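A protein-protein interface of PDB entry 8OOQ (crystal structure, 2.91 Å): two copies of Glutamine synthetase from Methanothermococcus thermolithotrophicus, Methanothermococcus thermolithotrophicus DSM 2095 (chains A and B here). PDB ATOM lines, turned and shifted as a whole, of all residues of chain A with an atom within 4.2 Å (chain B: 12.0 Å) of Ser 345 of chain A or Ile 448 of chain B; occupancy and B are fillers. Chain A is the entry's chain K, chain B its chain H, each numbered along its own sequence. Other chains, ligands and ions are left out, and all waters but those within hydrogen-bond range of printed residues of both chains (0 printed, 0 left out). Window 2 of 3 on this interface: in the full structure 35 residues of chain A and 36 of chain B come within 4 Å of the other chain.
Of the 12 printed residues of chain A, 5 touch a printed residue of chain B. Hydrophobic or aromatic side chains of chain B within 4 Å of the printed part of chain A: Tyr 445 and Ile 448. Among the printed residues, no Asp or Glu carboxylate lies within 4 Å of a Lys or Arg side-chain nitrogen of the other chain.
Among the printed residues, pairs that only touch across the chains: Thr 297 of chain A with Tyr 445 of chain B, Ser 345 of chain A with Ile 448 of chain B and Thr 235 of chain A with Tyr 445 of chain B.
Of the printed residues of chain B, Lys 224 of chain A touches Lys 447 (2.8 Å) and Ile 448 (3.3 Å). Thr 235 of chain A touches three residues of chain B. Of chain B, only Tyr 445 (3.6 Å) comes within 4 Å of Thr 297 of chain A. Ser 300 of chain A touches none of the printed residues of chain B. No residue of chain B comes within 4 Å of Pro 344 of chain A. Of chain B, only Ile 448 (3.6 Å) comes within 4 Å of Ser 345 of chain A. No residue of chain B comes within 4 Å of Cys 346 of chain A. Of the printed residues of chain A, Tyr 445 of chain B touches Thr 235 (3.9 Å) and Thr 297 (3.6 Å). Of the printed residues of chain A, Leu 446 of chain B touches Thr 235 (2.7 Å). Printed residues of chain A within 4 Å of Lys 447 of chain B: Lys 224 (2.8 Å). Of chain A, only Lys 224, Thr 235, Phe 236 and Ser 345 come within 4 Å of Ile 448 of chain B. The nearest residue of chain B that does not touch Ser 345 of chain A is Tyr 445 of chain B (6.4 Å). The nearest residue of chain A that does not touch Ile 448 of chain B is Thr 297 of chain A (4.1 Å). The nearest printed residue of chain B that does not touch Lys 224 of chain A is Leu 446 of chain B (4.4 Å).
The backbone carbonyl oxygen (O) of Leu 446 of chain B lies within hydrogen-bond range of the side-chain hydroxyl (OG1) of Thr 235 of chain A, 2.7 Å away. The side-chain amino group of Lys 224 of chain A sits at hydrogen-bond distance from the backbone carbonyl oxygen of Lys 447 of chain B, 2.8 Å away. O of Ile 448 of chain B is in salt-bridge range of NZ of Lys 224 of chain A, at 3.3 Å. The chain-end carboxylate (O) of Ile 448 of chain B is in hydrogen-bond range of the side-chain hydroxyl (OG1) of Thr 235 of chain A (3.3 Å). N of Phe 236 of chain A lies within hydrogen-bond range of O of Ile 448 of chain B (3.0 Å).
OG1 of Thr 297 of chain A lies within hydrogen-bond range of N of Ser 300 of chain A, 3.1 Å away. The side-chain hydroxyl of Ser 300 of chain A is in hydrogen-bond range of the side-chain hydroxyl of Ser 345 of chain A, at 3.5 Å. The side-chain hydroxyl (OG) of Ser 345 of chain A lies within hydrogen-bond range of the side-chain carboxylate (OD1) of Asp 343 of chain A (2.8 Å).
No position is printed for both chains. Of the 8 pairs that touch across the chains among the printed residues, none has its exchanged pair printed and touching as well.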
ATOM      1  N   LYS A 224     -15.115 -18.487  -9.992  1.00  0.00           N
ATOM      2  CA  LYS A 224     -15.122 -17.840  -8.678  1.00  0.00           C
ATOM      3  C   LYS A 224     -16.235 -18.333  -7.742  1.00  0.00           C
ATOM      4  O   LYS A 224     -15.980 -18.541  -6.551  1.00  0.00           O
ATOM      5  CB  LYS A 224     -15.221 -16.321  -8.843  1.00  0.00           C
ATOM      6  CG  LYS A 224     -14.018 -15.707  -9.531  1.00  0.00           C
ATOM      7  CD  LYS A 224     -14.247 -14.235  -9.794  1.00  0.00           C
ATOM      8  CE  LYS A 224     -12.978 -13.429  -9.722  1.00  0.00           C
ATOM      9  NZ  LYS A 224     -12.467 -13.282  -8.327  1.00  0.00           N
ATOM     10  N   THR A 235      -8.825 -16.326  -8.253  1.00  0.00           N
ATOM     11  CA  THR A 235      -8.440 -15.022  -8.789  1.00  0.00           C
ATOM     12  C   THR A 235      -7.854 -15.131 -10.196  1.00  0.00           C
ATOM     13  O   THR A 235      -7.005 -15.983 -10.462  1.00  0.00           O
ATOM     14  CB  THR A 235      -7.446 -14.304  -7.852  1.00  0.00           C
ATOM     15  OG1 THR A 235      -7.208 -12.989  -8.354  1.00  0.00           O
ATOM     16  CG2 THR A 235      -6.111 -15.031  -7.715  1.00  0.00           C
ATOM     17  N   PHE A 236      -8.290 -14.238 -11.086  1.00  0.00           N
ATOM     18  CA  PHE A 236      -7.767 -14.146 -12.444  1.00  0.00           C
ATOM     19  C   PHE A 236      -6.760 -12.984 -12.508  1.00  0.00           C
ATOM     20  O   PHE A 236      -6.706 -12.271 -13.507  1.00  0.00           O
ATOM     21  CB  PHE A 236      -8.914 -13.923 -13.436  1.00  0.00           C
ATOM     22  CG  PHE A 236      -9.790 -15.132 -13.635  1.00  0.00           C
ATOM     23  CD1 PHE A 236     -10.886 -15.356 -12.822  1.00  0.00           C
ATOM     24  CD2 PHE A 236      -9.529 -16.038 -14.646  1.00  0.00           C
ATOM     25  CE1 PHE A 236     -11.689 -16.468 -13.008  1.00  0.00           C
ATOM     26  CE2 PHE A 236     -10.348 -17.137 -14.845  1.00  0.00           C
ATOM     27  CZ  PHE A 236     -11.419 -17.346 -14.023  1.00  0.00           C
ATOM     28  N   PRO A 238      -3.270 -11.335 -13.201  1.00  0.00           N
ATOM     29  CA  PRO A 238      -2.163 -11.786 -14.067  1.00  0.00           C
ATOM     30  C   PRO A 238      -0.882 -12.255 -13.371  1.00  0.00           C
ATOM     31  O   PRO A 238      -0.095 -12.955 -13.991  1.00  0.00           O
ATOM     32  CB  PRO A 238      -1.855 -10.559 -14.924  1.00  0.00           C
ATOM     33  CG  PRO A 238      -3.055  -9.714 -14.855  1.00  0.00           C
ATOM     34  CD  PRO A 238      -3.667  -9.950 -13.519  1.00  0.00           C
ATOM     35  N   PRO A 296      -4.752  -4.781 -19.478  1.00  0.00           N
ATOM     36  CA  PRO A 296      -5.123  -3.449 -18.972  1.00  0.00           C
ATOM     37  C   PRO A 296      -4.805  -3.120 -17.516  1.00  0.00           C
ATOM     38  O   PRO A 296      -5.114  -2.013 -17.089  1.00  0.00           O
ATOM     39  CB  PRO A 296      -6.629  -3.436 -19.198  1.00  0.00           C
ATOM     40  CG  PRO A 296      -7.035  -4.805 -18.935  1.00  0.00           C
ATOM     41  CD  PRO A 296      -5.908  -5.694 -19.433  1.00  0.00           C
ATOM     42  N   THR A 297      -4.211  -4.038 -16.751  1.00  0.00           N
ATOM     43  CA  THR A 297      -3.902  -3.778 -15.345  1.00  0.00           C
ATOM     44  C   THR A 297      -2.431  -3.418 -15.150  1.00  0.00           C
ATOM     45  O   THR A 297      -1.600  -3.720 -16.005  1.00  0.00           O
ATOM     46  CB  THR A 297      -4.290  -4.998 -14.512  1.00  0.00           C
ATOM     47  OG1 THR A 297      -3.445  -6.096 -14.855  1.00  0.00           O
ATOM     48  CG2 THR A 297      -5.749  -5.380 -14.696  1.00  0.00           C
ATOM     49  N   SER A 300      -0.441  -6.632 -14.856  1.00  0.00           N
ATOM     50  CA  SER A 300      -0.196  -7.366 -16.096  1.00  0.00           C
ATOM     51  C   SER A 300       1.238  -7.220 -16.590  1.00  0.00           C
ATOM     52  O   SER A 300       1.757  -8.148 -17.201  1.00  0.00           O
ATOM     53  CB  SER A 300      -1.148  -6.905 -17.188  1.00  0.00           C
ATOM     54  OG  SER A 300      -2.507  -7.029 -16.799  1.00  0.00           O
ATOM     55  N   ASP A 343      -3.915 -11.762 -20.846  1.00  0.00           N
ATOM     56  CA  ASP A 343      -4.143 -12.334 -19.495  1.00  0.00           C
ATOM     57  C   ASP A 343      -5.653 -12.266 -19.234  1.00  0.00           C
ATOM     58  O   ASP A 343      -6.330 -11.419 -19.829  1.00  0.00           O
ATOM     59  CB  ASP A 343      -3.339 -11.587 -18.429  1.00  0.00           C
ATOM     60  CG  ASP A 343      -3.395 -10.076 -18.576  1.00  0.00           C
ATOM     61  OD1 ASP A 343      -4.443  -9.570 -19.023  1.00  0.00           O
ATOM     62  OD2 ASP A 343      -2.389  -9.418 -18.243  1.00  0.00           O
ATOM     63  N   PRO A 344      -6.223 -13.112 -18.349  1.00  0.00           N
ATOM     64  CA  PRO A 344      -7.680 -13.062 -18.135  1.00  0.00           C
ATOM     65  C   PRO A 344      -8.234 -11.782 -17.481  1.00  0.00           C
ATOM     66  O   PRO A 344      -9.442 -11.698 -17.277  1.00  0.00           O
ATOM     67  CB  PRO A 344      -7.947 -14.308 -17.295  1.00  0.00           C
ATOM     68  CG  PRO A 344      -6.673 -14.559 -16.580  1.00  0.00           C
ATOM     69  CD  PRO A 344      -5.613 -14.214 -17.576  1.00  0.00           C
ATOM     70  N   SER A 345      -7.392 -10.764 -17.222  1.00  0.00           N
ATOM     71  CA  SER A 345      -7.851  -9.491 -16.662  1.00  0.00           C
ATOM     72  C   SER A 345      -8.505  -8.564 -17.711  1.00  0.00           C
ATOM     73  O   SER A 345      -9.117  -7.569 -17.326  1.00  0.00           O
ATOM     74  CB  SER A 345      -6.683  -8.759 -16.010  1.00  0.00           C
ATOM     75  OG  SER A 345      -5.792  -8.181 -16.949  1.00  0.00           O
ATOM     76  N   CYS A 346      -8.360  -8.865 -19.020  1.00  0.00           N
ATOM     77  CA  CYS A 346      -8.898  -8.027 -20.089  1.00  0.00           C
ATOM     78  C   CYS A 346     -10.371  -8.275 -20.383  1.00  0.00           C
ATOM     79  O   CYS A 346     -10.902  -9.340 -20.072  1.00  0.00           O
ATOM     80  CB  CYS A 346      -8.052  -8.183 -21.348  1.00  0.00           C
ATOM     81  SG  CYS A 346      -8.264  -9.770 -22.193  1.00  0.00           S
ATOM     82  N   ASN A 347     -11.025  -7.281 -21.001  1.00  0.00           N
ATOM     83  CA  ASN A 347     -12.416  -7.386 -21.422  1.00  0.00           C
ATOM     84  C   ASN A 347     -12.379  -8.232 -22.699  1.00  0.00           C
ATOM     85  O   ASN A 347     -11.728  -7.805 -23.652  1.00  0.00           O
ATOM     86  CB  ASN A 347     -12.982  -5.991 -21.713  1.00  0.00           C
ATOM     87  CG  ASN A 347     -14.444  -5.964 -22.096  1.00  0.00           C
ATOM     88  OD1 ASN A 347     -15.010  -6.934 -22.599  1.00  0.00           O
ATOM     89  ND2 ASN A 347     -15.095  -4.841 -21.860  1.00  0.00           N
ATOM     90  N   VAL B 437       5.661  -7.831  -7.218  1.00  0.00           N
ATOM     91  CA  VAL B 437       4.214  -7.662  -7.096  1.00  0.00           C
ATOM     92  C   VAL B 437       3.977  -6.835  -5.830  1.00  0.00           C
ATOM     93  O   VAL B 437       4.269  -7.299  -4.731  1.00  0.00           O
ATOM     94  CB  VAL B 437       3.493  -9.029  -7.041  1.00  0.00           C
ATOM     95  CG1 VAL B 437       1.995  -8.848  -6.817  1.00  0.00           C
ATOM     96  CG2 VAL B 437       3.754  -9.828  -8.311  1.00  0.00           C
ATOM     97  N   TRP B 440      -0.266  -2.611  -3.539  1.00  0.00           N
ATOM     98  CA  TRP B 440      -1.300  -1.854  -4.244  1.00  0.00           C
ATOM     99  C   TRP B 440      -1.968  -2.754  -5.285  1.00  0.00           C
ATOM    100  O   TRP B 440      -3.195  -2.772  -5.380  1.00  0.00           O
ATOM    101  CB  TRP B 440      -0.689  -0.616  -4.929  1.00  0.00           C
ATOM    102  CG  TRP B 440      -1.696   0.289  -5.576  1.00  0.00           C
ATOM    103  CD1 TRP B 440      -2.296   1.377  -5.017  1.00  0.00           C
ATOM    104  CD2 TRP B 440      -2.170   0.219  -6.929  1.00  0.00           C
ATOM    105  NE1 TRP B 440      -3.132   1.977  -5.930  1.00  0.00           N
ATOM    106  CE2 TRP B 440      -3.080   1.279  -7.109  1.00  0.00           C
ATOM    107  CE3 TRP B 440      -1.941  -0.658  -7.996  1.00  0.00           C
ATOM    108  CZ2 TRP B 440      -3.741   1.496  -8.316  1.00  0.00           C
ATOM    109  CZ3 TRP B 440      -2.596  -0.439  -9.190  1.00  0.00           C
ATOM    110  CH2 TRP B 440      -3.485   0.624  -9.341  1.00  0.00           C
ATOM    111  N   GLU B 441      -1.157  -3.496  -6.063  1.00  0.00           N
ATOM    112  CA  GLU B 441      -1.655  -4.411  -7.090  1.00  0.00           C
ATOM    113  C   GLU B 441      -2.505  -5.512  -6.469  1.00  0.00           C
ATOM    114  O   GLU B 441      -3.546  -5.850  -7.014  1.00  0.00           O
ATOM    115  CB  GLU B 441      -0.491  -5.059  -7.850  1.00  0.00           C
ATOM    116  CG  GLU B 441       0.279  -4.123  -8.756  1.00  0.00           C
ATOM    117  CD  GLU B 441       1.645  -4.675  -9.107  1.00  0.00           C
ATOM    118  OE1 GLU B 441       1.717  -5.820  -9.609  1.00  0.00           O
ATOM    119  OE2 GLU B 441       2.651  -3.985  -8.826  1.00  0.00           O
ATOM    120  N   THR B 442      -2.064  -6.080  -5.340  1.00  0.00           N
ATOM    121  CA  THR B 442      -2.815  -7.135  -4.668  1.00  0.00           C
ATOM    122  C   THR B 442      -4.170  -6.609  -4.197  1.00  0.00           C
ATOM    123  O   THR B 442      -5.175  -7.294  -4.351  1.00  0.00           O
ATOM    124  CB  THR B 442      -1.987  -7.720  -3.519  1.00  0.00           C
ATOM    125  OG1 THR B 442      -0.725  -8.143  -4.036  1.00  0.00           O
ATOM    126  CG2 THR B 442      -2.685  -8.885  -2.834  1.00  0.00           C
ATOM    127  N   THR B 443      -4.202  -5.384  -3.667  1.00  0.00           N
ATOM    128  CA  THR B 443      -5.449  -4.778  -3.207  1.00  0.00           C
ATOM    129  C   THR B 443      -6.403  -4.510  -4.377  1.00  0.00           C
ATOM    130  O   THR B 443      -7.595  -4.796  -4.275  1.00  0.00           O
ATOM    131  CB  THR B 443      -5.146  -3.477  -2.447  1.00  0.00           C
ATOM    132  OG1 THR B 443      -4.257  -3.759  -1.365  1.00  0.00           O
ATOM    133  CG2 THR B 443      -6.401  -2.808  -1.919  1.00  0.00           C
ATOM    134  N   ALA B 444      -5.877  -3.975  -5.484  1.00  0.00           N
ATOM    135  CA  ALA B 444      -6.684  -3.611  -6.645  1.00  0.00           C
ATOM    136  C   ALA B 444      -7.089  -4.748  -7.587  1.00  0.00           C
ATOM    137  O   ALA B 444      -8.135  -4.630  -8.221  1.00  0.00           O
ATOM    138  CB  ALA B 444      -5.953  -2.545  -7.447  1.00  0.00           C
ATOM    139  N   TYR B 445      -6.272  -5.805  -7.731  1.00  0.00           N
ATOM    140  CA  TYR B 445      -6.536  -6.853  -8.722  1.00  0.00           C
ATOM    141  C   TYR B 445      -6.791  -8.270  -8.197  1.00  0.00           C
ATOM    142  O   TYR B 445      -7.135  -9.117  -9.020  1.00  0.00           O
ATOM    143  CB  TYR B 445      -5.377  -6.906  -9.733  1.00  0.00           C
ATOM    144  CG  TYR B 445      -5.048  -5.557 -10.332  1.00  0.00           C
ATOM    145  CD1 TYR B 445      -6.008  -4.824 -11.014  1.00  0.00           C
ATOM    146  CD2 TYR B 445      -3.788  -4.999 -10.187  1.00  0.00           C
ATOM    147  CE1 TYR B 445      -5.727  -3.562 -11.521  1.00  0.00           C
ATOM    148  CE2 TYR B 445      -3.487  -3.752 -10.713  1.00  0.00           C
ATOM    149  CZ  TYR B 445      -4.455  -3.038 -11.389  1.00  0.00           C
ATOM    150  OH  TYR B 445      -4.139  -1.807 -11.909  1.00  0.00           O
ATOM    151  N   LEU B 446      -6.647  -8.555  -6.887  1.00  0.00           N
ATOM    152  CA  LEU B 446      -6.927  -9.915  -6.397  1.00  0.00           C
ATOM    153  C   LEU B 446      -8.419 -10.258  -6.557  1.00  0.00           C
ATOM    154  O   LEU B 446      -8.759 -11.419  -6.785  1.00  0.00           O
ATOM    155  CB  LEU B 446      -6.499 -10.095  -4.933  1.00  0.00           C
ATOM    156  CG  LEU B 446      -6.302 -11.544  -4.456  1.00  0.00           C
ATOM    157  CD1 LEU B 446      -4.997 -12.132  -4.991  1.00  0.00           C
ATOM    158  CD2 LEU B 446      -6.317 -11.623  -2.942  1.00  0.00           C
ATOM    159  N   LYS B 447      -9.302  -9.254  -6.451  1.00  0.00           N
ATOM    160  CA  LYS B 447     -10.740  -9.443  -6.607  1.00  0.00           C
ATOM    161  C   LYS B 447     -11.157  -9.836  -8.032  1.00  0.00           C
ATOM    162  O   LYS B 447     -12.206 -10.459  -8.192  1.00  0.00           O
ATOM    163  CB  LYS B 447     -11.488  -8.165  -6.187  1.00  0.00           C
ATOM    164  CG  LYS B 447     -11.306  -6.986  -7.145  1.00  0.00           C
ATOM    165  CD  LYS B 447     -11.585  -5.654  -6.467  1.00  0.00           C
ATOM    166  CE  LYS B 447     -11.474  -4.495  -7.428  1.00  0.00           C
ATOM    167  NZ  LYS B 447     -11.684  -3.192  -6.746  1.00  0.00           N
ATOM    168  N   ILE B 448     -10.364  -9.474  -9.061  1.00  0.00           N
ATOM    169  CA  ILE B 448     -10.724  -9.782 -10.453  1.00  0.00           C
ATOM    170  C   ILE B 448     -10.492 -11.258 -10.806  1.00  0.00           C
ATOM    171  O   ILE B 448      -9.877 -11.998 -10.004  1.00  0.00           O
ATOM    172  CB  ILE B 448     -10.026  -8.819 -11.470  1.00  0.00           C
ATOM    173  CG1 ILE B 448      -8.537  -9.208 -11.723  1.00  0.00           C
ATOM    174  CG2 ILE B 448     -10.192  -7.355 -11.019  1.00  0.00           C
ATOM    175  CD1 ILE B 448      -7.728  -8.244 -12.560  1.00  0.00           C
ATOM    176  OXT ILE B 448     -10.927 -11.669 -11.904  1.00  0.00           O
